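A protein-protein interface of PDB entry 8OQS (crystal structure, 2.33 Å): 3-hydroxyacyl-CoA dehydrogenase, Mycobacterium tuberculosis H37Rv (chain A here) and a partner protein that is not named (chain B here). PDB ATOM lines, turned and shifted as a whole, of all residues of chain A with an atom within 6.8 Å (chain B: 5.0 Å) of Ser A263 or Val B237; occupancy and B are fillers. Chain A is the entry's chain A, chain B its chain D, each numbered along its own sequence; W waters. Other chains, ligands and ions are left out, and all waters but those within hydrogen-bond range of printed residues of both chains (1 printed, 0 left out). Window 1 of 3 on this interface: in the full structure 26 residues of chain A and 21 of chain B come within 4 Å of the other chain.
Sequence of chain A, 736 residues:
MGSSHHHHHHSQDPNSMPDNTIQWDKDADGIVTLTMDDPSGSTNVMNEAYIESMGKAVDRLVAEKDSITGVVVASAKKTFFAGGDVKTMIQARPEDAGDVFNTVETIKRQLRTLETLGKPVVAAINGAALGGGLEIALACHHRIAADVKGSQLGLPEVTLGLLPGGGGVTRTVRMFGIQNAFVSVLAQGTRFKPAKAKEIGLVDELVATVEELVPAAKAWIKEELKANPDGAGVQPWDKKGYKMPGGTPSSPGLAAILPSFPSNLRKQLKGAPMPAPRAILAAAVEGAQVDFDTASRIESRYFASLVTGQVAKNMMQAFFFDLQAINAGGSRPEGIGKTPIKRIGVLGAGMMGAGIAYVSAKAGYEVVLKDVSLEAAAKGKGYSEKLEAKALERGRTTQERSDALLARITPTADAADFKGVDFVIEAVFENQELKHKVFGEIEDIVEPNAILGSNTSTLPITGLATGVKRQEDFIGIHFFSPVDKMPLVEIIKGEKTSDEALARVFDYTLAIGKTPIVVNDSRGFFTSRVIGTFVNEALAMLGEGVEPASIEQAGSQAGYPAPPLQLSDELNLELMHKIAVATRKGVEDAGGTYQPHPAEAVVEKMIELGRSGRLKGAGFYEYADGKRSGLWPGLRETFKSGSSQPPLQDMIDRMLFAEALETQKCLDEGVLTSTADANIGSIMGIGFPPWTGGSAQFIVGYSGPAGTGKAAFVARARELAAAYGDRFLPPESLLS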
ATOM      1  N   LEU A 258      10.497 -11.421  15.552  1.00  0.00           N
ATOM      2  CA  LEU A 258      10.560 -11.394  14.093  1.00  0.00           C
ATOM      3  C   LEU A 258       9.213 -11.166  13.411  1.00  0.00           C
ATOM      4  O   LEU A 258       9.191 -10.456  12.391  1.00  0.00           O
ATOM      5  CB  LEU A 258      11.207 -12.686  13.587  1.00  0.00           C
ATOM      6  CG  LEU A 258      11.717 -12.671  12.148  1.00  0.00           C
ATOM      7  CD1 LEU A 258      12.582 -11.449  11.917  1.00  0.00           C
ATOM      8  CD2 LEU A 258      12.506 -13.935  11.867  1.00  0.00           C
ATOM      9  N   PRO A 259       8.087 -11.721  13.878  1.00  0.00           N
ATOM     10  CA  PRO A 259       6.806 -11.423  13.210  1.00  0.00           C
ATOM     11  C   PRO A 259       6.389  -9.968  13.290  1.00  0.00           C
ATOM     12  O   PRO A 259       5.574  -9.530  12.468  1.00  0.00           O
ATOM     13  CB  PRO A 259       5.806 -12.325  13.947  1.00  0.00           C
ATOM     14  CG  PRO A 259       6.624 -13.432  14.462  1.00  0.00           C
ATOM     15  CD  PRO A 259       7.930 -12.815  14.852  1.00  0.00           C
ATOM     16  N   SER A 260       6.905  -9.205  14.251  1.00  0.00           N
ATOM     17  CA  SER A 260       6.556  -7.795  14.342  1.00  0.00           C
ATOM     18  C   SER A 260       7.322  -6.929  13.353  1.00  0.00           C
ATOM     19  O   SER A 260       6.990  -5.746  13.210  1.00  0.00           O
ATOM     20  CB  SER A 260       6.805  -7.274  15.759  1.00  0.00           C
ATOM     21  OG  SER A 260       8.185  -7.031  15.968  1.00  0.00           O
ATOM     22  N   PHE A 261       8.341  -7.476  12.675  1.00  0.00           N
ATOM     23  CA  PHE A 261       9.106  -6.654  11.738  1.00  0.00           C
ATOM     24  C   PHE A 261       8.272  -6.235  10.534  1.00  0.00           C
ATOM     25  O   PHE A 261       8.279  -5.040  10.195  1.00  0.00           O
ATOM     26  CB  PHE A 261      10.389  -7.378  11.319  1.00  0.00           C
ATOM     27  CG  PHE A 261      11.437  -7.455  12.404  1.00  0.00           C
ATOM     28  CD1 PHE A 261      11.191  -6.953  13.674  1.00  0.00           C
ATOM     29  CD2 PHE A 261      12.673  -8.029  12.148  1.00  0.00           C
ATOM     30  CE1 PHE A 261      12.152  -7.030  14.669  1.00  0.00           C
ATOM     31  CE2 PHE A 261      13.643  -8.110  13.139  1.00  0.00           C
ATOM     32  CZ  PHE A 261      13.381  -7.606  14.400  1.00  0.00           C
ATOM     33  N   PRO A 262       7.539  -7.125   9.852  1.00  0.00           N
ATOM     34  CA  PRO A 262       6.698  -6.647   8.743  1.00  0.00           C
ATOM     35  C   PRO A 262       5.548  -5.772   9.199  1.00  0.00           C
ATOM     36  O   PRO A 262       5.147  -4.868   8.455  1.00  0.00           O
ATOM     37  CB  PRO A 262       6.191  -7.944   8.097  1.00  0.00           C
ATOM     38  CG  PRO A 262       7.159  -8.987   8.526  1.00  0.00           C
ATOM     39  CD  PRO A 262       7.536  -8.598   9.918  1.00  0.00           C
ATOM     40  N   SER A 263       4.997  -6.011  10.392  1.00  0.00           N
ATOM     41  CA  SER A 263       3.901  -5.177  10.870  1.00  0.00           C
ATOM     42  C   SER A 263       4.384  -3.771  11.206  1.00  0.00           C
ATOM     43  O   SER A 263       3.719  -2.786  10.869  1.00  0.00           O
ATOM     44  CB  SER A 263       3.241  -5.827  12.082  1.00  0.00           C
ATOM     45  OG  SER A 263       4.156  -5.927  13.158  1.00  0.00           O
ATOM     46  N   ASN A 264       5.539  -3.654  11.870  1.00  0.00           N
ATOM     47  CA  ASN A 264       6.094  -2.331  12.133  1.00  0.00           C
ATOM     48  C   ASN A 264       6.423  -1.597  10.843  1.00  0.00           C
ATOM     49  O   ASN A 264       6.300  -0.370  10.787  1.00  0.00           O
ATOM     50  CB  ASN A 264       7.340  -2.434  13.012  1.00  0.00           C
ATOM     51  CG  ASN A 264       7.002  -2.525  14.488  1.00  0.00           C
ATOM     52  OD1 ASN A 264       6.518  -1.560  15.087  1.00  0.00           O
ATOM     53  ND2 ASN A 264       7.260  -3.686  15.085  1.00  0.00           N
ATOM     54  N   LEU A 265       6.834  -2.324   9.798  1.00  0.00           N
ATOM     55  CA  LEU A 265       7.070  -1.696   8.501  1.00  0.00           C
ATOM     56  C   LEU A 265       5.770  -1.173   7.899  1.00  0.00           C
ATOM     57  O   LEU A 265       5.709  -0.028   7.434  1.00  0.00           O
ATOM     58  CB  LEU A 265       7.746  -2.688   7.551  1.00  0.00           C
ATOM     59  CG  LEU A 265       8.212  -2.137   6.201  1.00  0.00           C
ATOM     60  CD1 LEU A 265       9.196  -0.995   6.404  1.00  0.00           C
ATOM     61  CD2 LEU A 265       8.834  -3.238   5.349  1.00  0.00           C
ATOM     62  N   ARG A 266       4.717  -2.001   7.895  1.00  0.00           N
ATOM     63  CA  ARG A 266       3.408  -1.535   7.442  1.00  0.00           C
ATOM     64  C   ARG A 266       2.947  -0.321   8.232  1.00  0.00           C
ATOM     65  O   ARG A 266       2.317   0.585   7.676  1.00  0.00           O
ATOM     66  CB  ARG A 266       2.368  -2.647   7.559  1.00  0.00           C
ATOM     67  CG  ARG A 266       2.546  -3.774   6.571  1.00  0.00           C
ATOM     68  CD  ARG A 266       1.273  -4.598   6.461  1.00  0.00           C
ATOM     69  NE  ARG A 266       0.279  -3.944   5.621  1.00  0.00           N
ATOM     70  CZ  ARG A 266      -0.077  -4.371   4.418  1.00  0.00           C
ATOM     71  NH1 ARG A 266       0.438  -5.470   3.895  1.00  0.00           N
ATOM     72  NH2 ARG A 266      -0.976  -3.677   3.723  1.00  0.00           N
ATOM     73  N   LYS A 267       3.242  -0.288   9.533  1.00  0.00           N
ATOM     74  CA  LYS A 267       2.865   0.866  10.341  1.00  0.00           C
ATOM     75  C   LYS A 267       3.637   2.109   9.918  1.00  0.00           C
ATOM     76  O   LYS A 267       3.052   3.189   9.777  1.00  0.00           O
ATOM     77  CB  LYS A 267       3.082   0.560  11.823  1.00  0.00           C
ATOM     78  CG  LYS A 267       3.088   1.784  12.727  1.00  0.00           C
ATOM     79  CD  LYS A 267       2.855   1.389  14.178  1.00  0.00           C
ATOM     80  CE  LYS A 267       3.241   2.499  15.148  1.00  0.00           C
ATOM     81  NZ  LYS A 267       4.715   2.732  15.179  1.00  0.00           N
ATOM     82  N   GLN A 268       4.948   1.977   9.696  1.00  0.00           N
ATOM     83  CA  GLN A 268       5.753   3.118   9.268  1.00  0.00           C
ATOM     84  C   GLN A 268       5.329   3.609   7.888  1.00  0.00           C
ATOM     85  O   GLN A 268       5.147   4.812   7.677  1.00  0.00           O
ATOM     86  CB  GLN A 268       7.235   2.748   9.272  1.00  0.00           C
ATOM     87  CG  GLN A 268       7.799   2.443  10.651  1.00  0.00           C
ATOM     88  CD  GLN A 268       7.906   3.676  11.523  1.00  0.00           C
ATOM     89  OE1 GLN A 268       6.947   4.071  12.192  1.00  0.00           O
ATOM     90  NE2 GLN A 268       9.083   4.295  11.521  1.00  0.00           N
ATOM     91  N   LEU A 281      13.598  -6.158   3.546  1.00  0.00           N
ATOM     92  CA  LEU A 281      13.332  -6.965   4.733  1.00  0.00           C
ATOM     93  C   LEU A 281      13.284  -8.448   4.388  1.00  0.00           C
ATOM     94  O   LEU A 281      13.750  -9.288   5.168  1.00  0.00           O
ATOM     95  CB  LEU A 281      12.022  -6.519   5.380  1.00  0.00           C
ATOM     96  CG  LEU A 281      11.694  -7.174   6.717  1.00  0.00           C
ATOM     97  CD1 LEU A 281      12.820  -6.926   7.715  1.00  0.00           C
ATOM     98  CD2 LEU A 281      10.375  -6.644   7.244  1.00  0.00           C
ATOM     99  N   ASN B 141       4.327 -12.695   5.486  1.00  0.00           N
ATOM    100  CA  ASN B 141       3.738 -11.894   6.561  1.00  0.00           C
ATOM    101  C   ASN B 141       3.191 -10.572   6.031  1.00  0.00           C
ATOM    102  O   ASN B 141       2.028 -10.232   6.272  1.00  0.00           O
ATOM    103  CB  ASN B 141       4.790 -11.667   7.653  1.00  0.00           C
ATOM    104  CG  ASN B 141       4.235 -11.024   8.915  1.00  0.00           C
ATOM    105  OD1 ASN B 141       3.437 -10.088   8.862  1.00  0.00           O
ATOM    106  ND2 ASN B 141       4.673 -11.523  10.067  1.00  0.00           N
ATOM    107  N   MET B 145      -1.138 -10.053   5.821  1.00  0.00           N
ATOM    108  CA  MET B 145      -1.498  -9.149   6.914  1.00  0.00           C
ATOM    109  C   MET B 145      -1.657  -9.929   8.225  1.00  0.00           C
ATOM    110  O   MET B 145      -2.739 -10.034   8.809  1.00  0.00           O
ATOM    111  CB  MET B 145      -2.759  -8.346   6.566  1.00  0.00           C
ATOM    112  CG  MET B 145      -2.667  -7.615   5.222  1.00  0.00           C
ATOM    113  SD  MET B 145      -3.981  -6.413   4.909  1.00  0.00           S
ATOM    114  CE  MET B 145      -3.430  -5.019   5.891  1.00  0.00           C
ATOM    115  N   PHE B 146      -0.527 -10.481   8.665  1.00  0.00           N
ATOM    116  CA  PHE B 146      -0.498 -11.288   9.877  1.00  0.00           C
ATOM    117  C   PHE B 146      -0.831 -10.443  11.100  1.00  0.00           C
ATOM    118  O   PHE B 146      -0.294  -9.346  11.282  1.00  0.00           O
ATOM    119  CB  PHE B 146       0.873 -11.942  10.046  1.00  0.00           C
ATOM    120  CG  PHE B 146       1.045 -12.655  11.360  1.00  0.00           C
ATOM    121  CD1 PHE B 146       0.579 -13.949  11.525  1.00  0.00           C
ATOM    122  CD2 PHE B 146       1.672 -12.032  12.430  1.00  0.00           C
ATOM    123  CE1 PHE B 146       0.729 -14.607  12.726  1.00  0.00           C
ATOM    124  CE2 PHE B 146       1.826 -12.685  13.636  1.00  0.00           C
ATOM    125  CZ  PHE B 146       1.354 -13.974  13.784  1.00  0.00           C
ATOM    126  N   VAL B 147      -1.709 -10.971  11.946  1.00  0.00           N
ATOM    127  CA  VAL B 147      -2.149 -10.314  13.174  1.00  0.00           C
ATOM    128  C   VAL B 147      -2.353 -11.400  14.225  1.00  0.00           C
ATOM    129  O   VAL B 147      -2.918 -12.455  13.909  1.00  0.00           O
ATOM    130  CB  VAL B 147      -3.434  -9.502  12.937  1.00  0.00           C
ATOM    131  CG1 VAL B 147      -4.159  -9.255  14.237  1.00  0.00           C
ATOM    132  CG2 VAL B 147      -3.114  -8.179  12.259  1.00  0.00           C
ATOM    133  N   GLY B 232       4.779  -3.757  18.570  1.00  0.00           N
ATOM    134  CA  GLY B 232       3.999  -2.766  17.864  1.00  0.00           C
ATOM    135  C   GLY B 232       3.633  -3.172  16.449  1.00  0.00           C
ATOM    136  O   GLY B 232       4.192  -4.098  15.860  1.00  0.00           O
ATOM    137  N   GLY B 233       2.652  -2.454  15.905  1.00  0.00           N
ATOM    138  CA  GLY B 233       2.330  -2.549  14.498  1.00  0.00           C
ATOM    139  C   GLY B 233       1.013  -3.220  14.172  1.00  0.00           C
ATOM    140  O   GLY B 233       0.328  -2.810  13.230  1.00  0.00           O
ATOM    141  N   PHE B 234       0.641  -4.248  14.937  1.00  0.00           N
ATOM    142  CA  PHE B 234      -0.491  -5.076  14.536  1.00  0.00           C
ATOM    143  C   PHE B 234      -1.807  -4.307  14.575  1.00  0.00           C
ATOM    144  O   PHE B 234      -2.708  -4.587  13.776  1.00  0.00           O
ATOM    145  CB  PHE B 234      -0.567  -6.323  15.414  1.00  0.00           C
ATOM    146  CG  PHE B 234       0.649  -7.194  15.327  1.00  0.00           C
ATOM    147  CD1 PHE B 234       0.954  -7.863  14.152  1.00  0.00           C
ATOM    148  CD2 PHE B 234       1.487  -7.347  16.421  1.00  0.00           C
ATOM    149  CE1 PHE B 234       2.073  -8.667  14.068  1.00  0.00           C
ATOM    150  CE2 PHE B 234       2.609  -8.150  16.344  1.00  0.00           C
ATOM    151  CZ  PHE B 234       2.903  -8.812  15.169  1.00  0.00           C
ATOM    152  N   ASP B 235      -1.938  -3.336  15.481  1.00  0.00           N
ATOM    153  CA  ASP B 235      -3.142  -2.511  15.506  1.00  0.00           C
ATOM    154  C   ASP B 235      -3.296  -1.736  14.205  1.00  0.00           C
ATOM    155  O   ASP B 235      -4.384  -1.687  13.619  1.00  0.00           O
ATOM    156  CB  ASP B 235      -3.100  -1.556  16.697  1.00  0.00           C
ATOM    157  CG  ASP B 235      -3.616  -2.191  17.966  1.00  0.00           C
ATOM    158  OD1 ASP B 235      -4.718  -2.778  17.927  1.00  0.00           O
ATOM    159  OD2 ASP B 235      -2.917  -2.113  18.997  1.00  0.00           O
ATOM    160  N   ASP B 236      -2.208  -1.119  13.738  1.00  0.00           N
ATOM    161  CA  ASP B 236      -2.254  -0.389  12.478  1.00  0.00           C
ATOM    162  C   ASP B 236      -2.527  -1.325  11.309  1.00  0.00           C
ATOM    163  O   ASP B 236      -3.305  -0.989  10.409  1.00  0.00           O
ATOM    164  CB  ASP B 236      -0.947   0.372  12.270  1.00  0.00           C
ATOM    165  CG  ASP B 236      -0.675   1.370  13.379  1.00  0.00           C
ATOM    166  OD1 ASP B 236      -0.526   0.939  14.543  1.00  0.00           O
ATOM    167  OD2 ASP B 236      -0.613   2.586  13.088  1.00  0.00           O
ATOM    168  N   VAL B 237      -1.910  -2.509  11.314  1.00  0.00           N
ATOM    169  CA  VAL B 237      -2.110  -3.460  10.223  1.00  0.00           C
ATOM    170  C   VAL B 237      -3.567  -3.890  10.149  1.00  0.00           C
ATOM    171  O   VAL B 237      -4.143  -3.998   9.058  1.00  0.00           O
ATOM    172  CB  VAL B 237      -1.173  -4.669  10.389  1.00  0.00           C
ATOM    173  CG1 VAL B 237      -1.435  -5.693   9.301  1.00  0.00           C
ATOM    174  CG2 VAL B 237       0.269  -4.215  10.353  1.00  0.00           C
ATOM    175  N   ALA B 238      -4.193  -4.130  11.305  1.00  0.00           N
ATOM    176  CA  ALA B 238      -5.604  -4.503  11.318  1.00  0.00           C
ATOM    177  C   ALA B 238      -6.475  -3.386  10.758  1.00  0.00           C
ATOM    178  O   ALA B 238      -7.391  -3.643   9.968  1.00  0.00           O
ATOM    179  CB  ALA B 238      -6.045  -4.862  12.738  1.00  0.00           C
ATOM    180  N   LEU B 239      -6.201  -2.137  11.145  1.00  0.00           N
ATOM    181  CA  LEU B 239      -7.017  -1.022  10.682  1.00  0.00           C
ATOM    182  C   LEU B 239      -6.742  -0.659   9.229  1.00  0.00           C
ATOM    183  O   LEU B 239      -7.571   0.011   8.603  1.00  0.00           O
ATOM    184  CB  LEU B 239      -6.800   0.201  11.570  1.00  0.00           C
ATOM    185  CG  LEU B 239      -7.221   0.039  13.027  1.00  0.00           C
ATOM    186  CD1 LEU B 239      -7.007   1.339  13.786  1.00  0.00           C
ATOM    187  CD2 LEU B 239      -8.667  -0.409  13.104  1.00  0.00           C
ATOM    188  N   GLN B 240      -5.595  -1.060   8.680  1.00  0.00           N
ATOM    189  CA  GLN B 240      -5.404  -0.906   7.243  1.00  0.00           C
ATOM    190  C   GLN B 240      -6.364  -1.802   6.473  1.00  0.00           C
ATOM    191  O   GLN B 240      -6.799  -1.443   5.373  1.00  0.00           O
ATOM    192  CB  GLN B 240      -3.953  -1.200   6.864  1.00  0.00           C
ATOM    193  CG  GLN B 240      -2.945  -0.178   7.386  1.00  0.00           C
ATOM    194  CD  GLN B 240      -1.523  -0.500   6.960  1.00  0.00           C
ATOM    195  OE1 GLN B 240      -1.290  -1.451   6.217  1.00  0.00           O
ATOM    196  NE2 GLN B 240      -0.564   0.292   7.432  1.00  0.00           N
ATOM    197  N   LYS B 241      -6.725  -2.953   7.050  1.00  0.00           N
ATOM    198  CA  LYS B 241      -7.723  -3.836   6.450  1.00  0.00           C
ATOM    199  C   LYS B 241      -9.139  -3.345   6.730  1.00  0.00           C
ATOM    200  O   LYS B 241      -9.963  -3.249   5.813  1.00  0.00           O
ATOM    201  CB  LYS B 241      -7.534  -5.260   6.976  1.00  0.00           C
ATOM    202  CG  LYS B 241      -8.620  -6.240   6.569  1.00  0.00           C
ATOM    203  CD  LYS B 241      -8.429  -6.736   5.153  1.00  0.00           C
ATOM    204  CE  LYS B 241      -9.529  -7.713   4.775  1.00  0.00           C
ATOM    205  NZ  LYS B 241      -9.337  -8.285   3.414  1.00  0.00           N
HETATM  206  O   HOH W   1       0.146   3.737  10.558  1.00  0.00           O
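Pro A259 touches Phe B234.
Ser A260 touches Phe B234.
Asn B141 touches Pro A262 (OD1 to CB, 3.6 Å).
O of Ser A263 touches CA of Gly B233, 3.9 Å away.
Ser A263 touches Phe B234.
O of Ser A263 touches CG2 of Val B237 (3.8 Å).
Met B145 touches Arg A266.
CG2 of Val B237 touches CB of Arg A266 (3.8 Å).
CD of Lys A267 touches CA of Gly B233 (3.99 Å).
Lys A267 touches Asp B236.
The backbone carbonyl oxygen (O) of Ser A260 sits at hydrogen-bond distance from the side-chain amide nitrogen (ND2) of Asn A264 (2.8 Å).
The backbone carbonyl oxygen of Ser A260 sits at hydrogen-bond distance from the side-chain hydroxyl of Ser A263 (2.8 Å).
Ser A263 touches just these residues of chain B: Gly B232 (3.3 Å), Gly B233 (3.9 Å), Phe B234 (3.6 Å) and Val B237 (3.8 Å).
Of the printed residues of chain A, Val B237 touches Ser A263 (3.8 Å) and Arg A266 (3.8 Å).
Of the printed residues of chain A, Met B145 touches Arg A266.
Of the printed residues of chain A, Phe B234 touches Pro A259, Ser A260 and Ser A263.
Of the printed residues of chain B, Pro A259 touches Asn B141 (3.2 Å) and Phe B234 (3.9 Å).
Of the printed residues of chain A, Gly B233 touches Ser A263 and Lys A267.
The nearest printed residue of chain B that does not touch Ser A260 is Gly B232 (4.1 Å).
Of the 12 printed residues of chain A, 7 touch a printed residue of chain B.
Hydrophobic or aromatic side chains of chain A that line the printed part of chain B: Pro A262.
Of the 14 printed residues of chain B, 8 touch a printed residue of chain A.
Hydrophobic or aromatic side chains of chain B that line the printed part of chain A: Met B145, Phe B234 and Val B237.
Among the printed residues, no Asp or Glu carboxylate lies within 4 Å of a Lys or Arg side-chain nitrogen of the other chain.
Water W1 bridges OD2 of Asp B236 (2.9 Å) and O of Lys A267 (3.1 Å).
The side-chain amide nitrogen (ND2) of Asn A264 is in hydrogen-bond range of the backbone carbonyl oxygen (O) of Gly B232, 3.2 Å away.
OG of Ser A263 is in hydrogen-bond range of O of Gly B232 (3.3 Å).
The backbone carbonyl oxygen (O) of Pro A259 sits at hydrogen-bond distance from the side-chain amide nitrogen (ND2) of Asn B141 (3.2 Å).
O of Arg A266 lies within hydrogen-bond range of NE2 of Gln B240 (2.9 Å).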
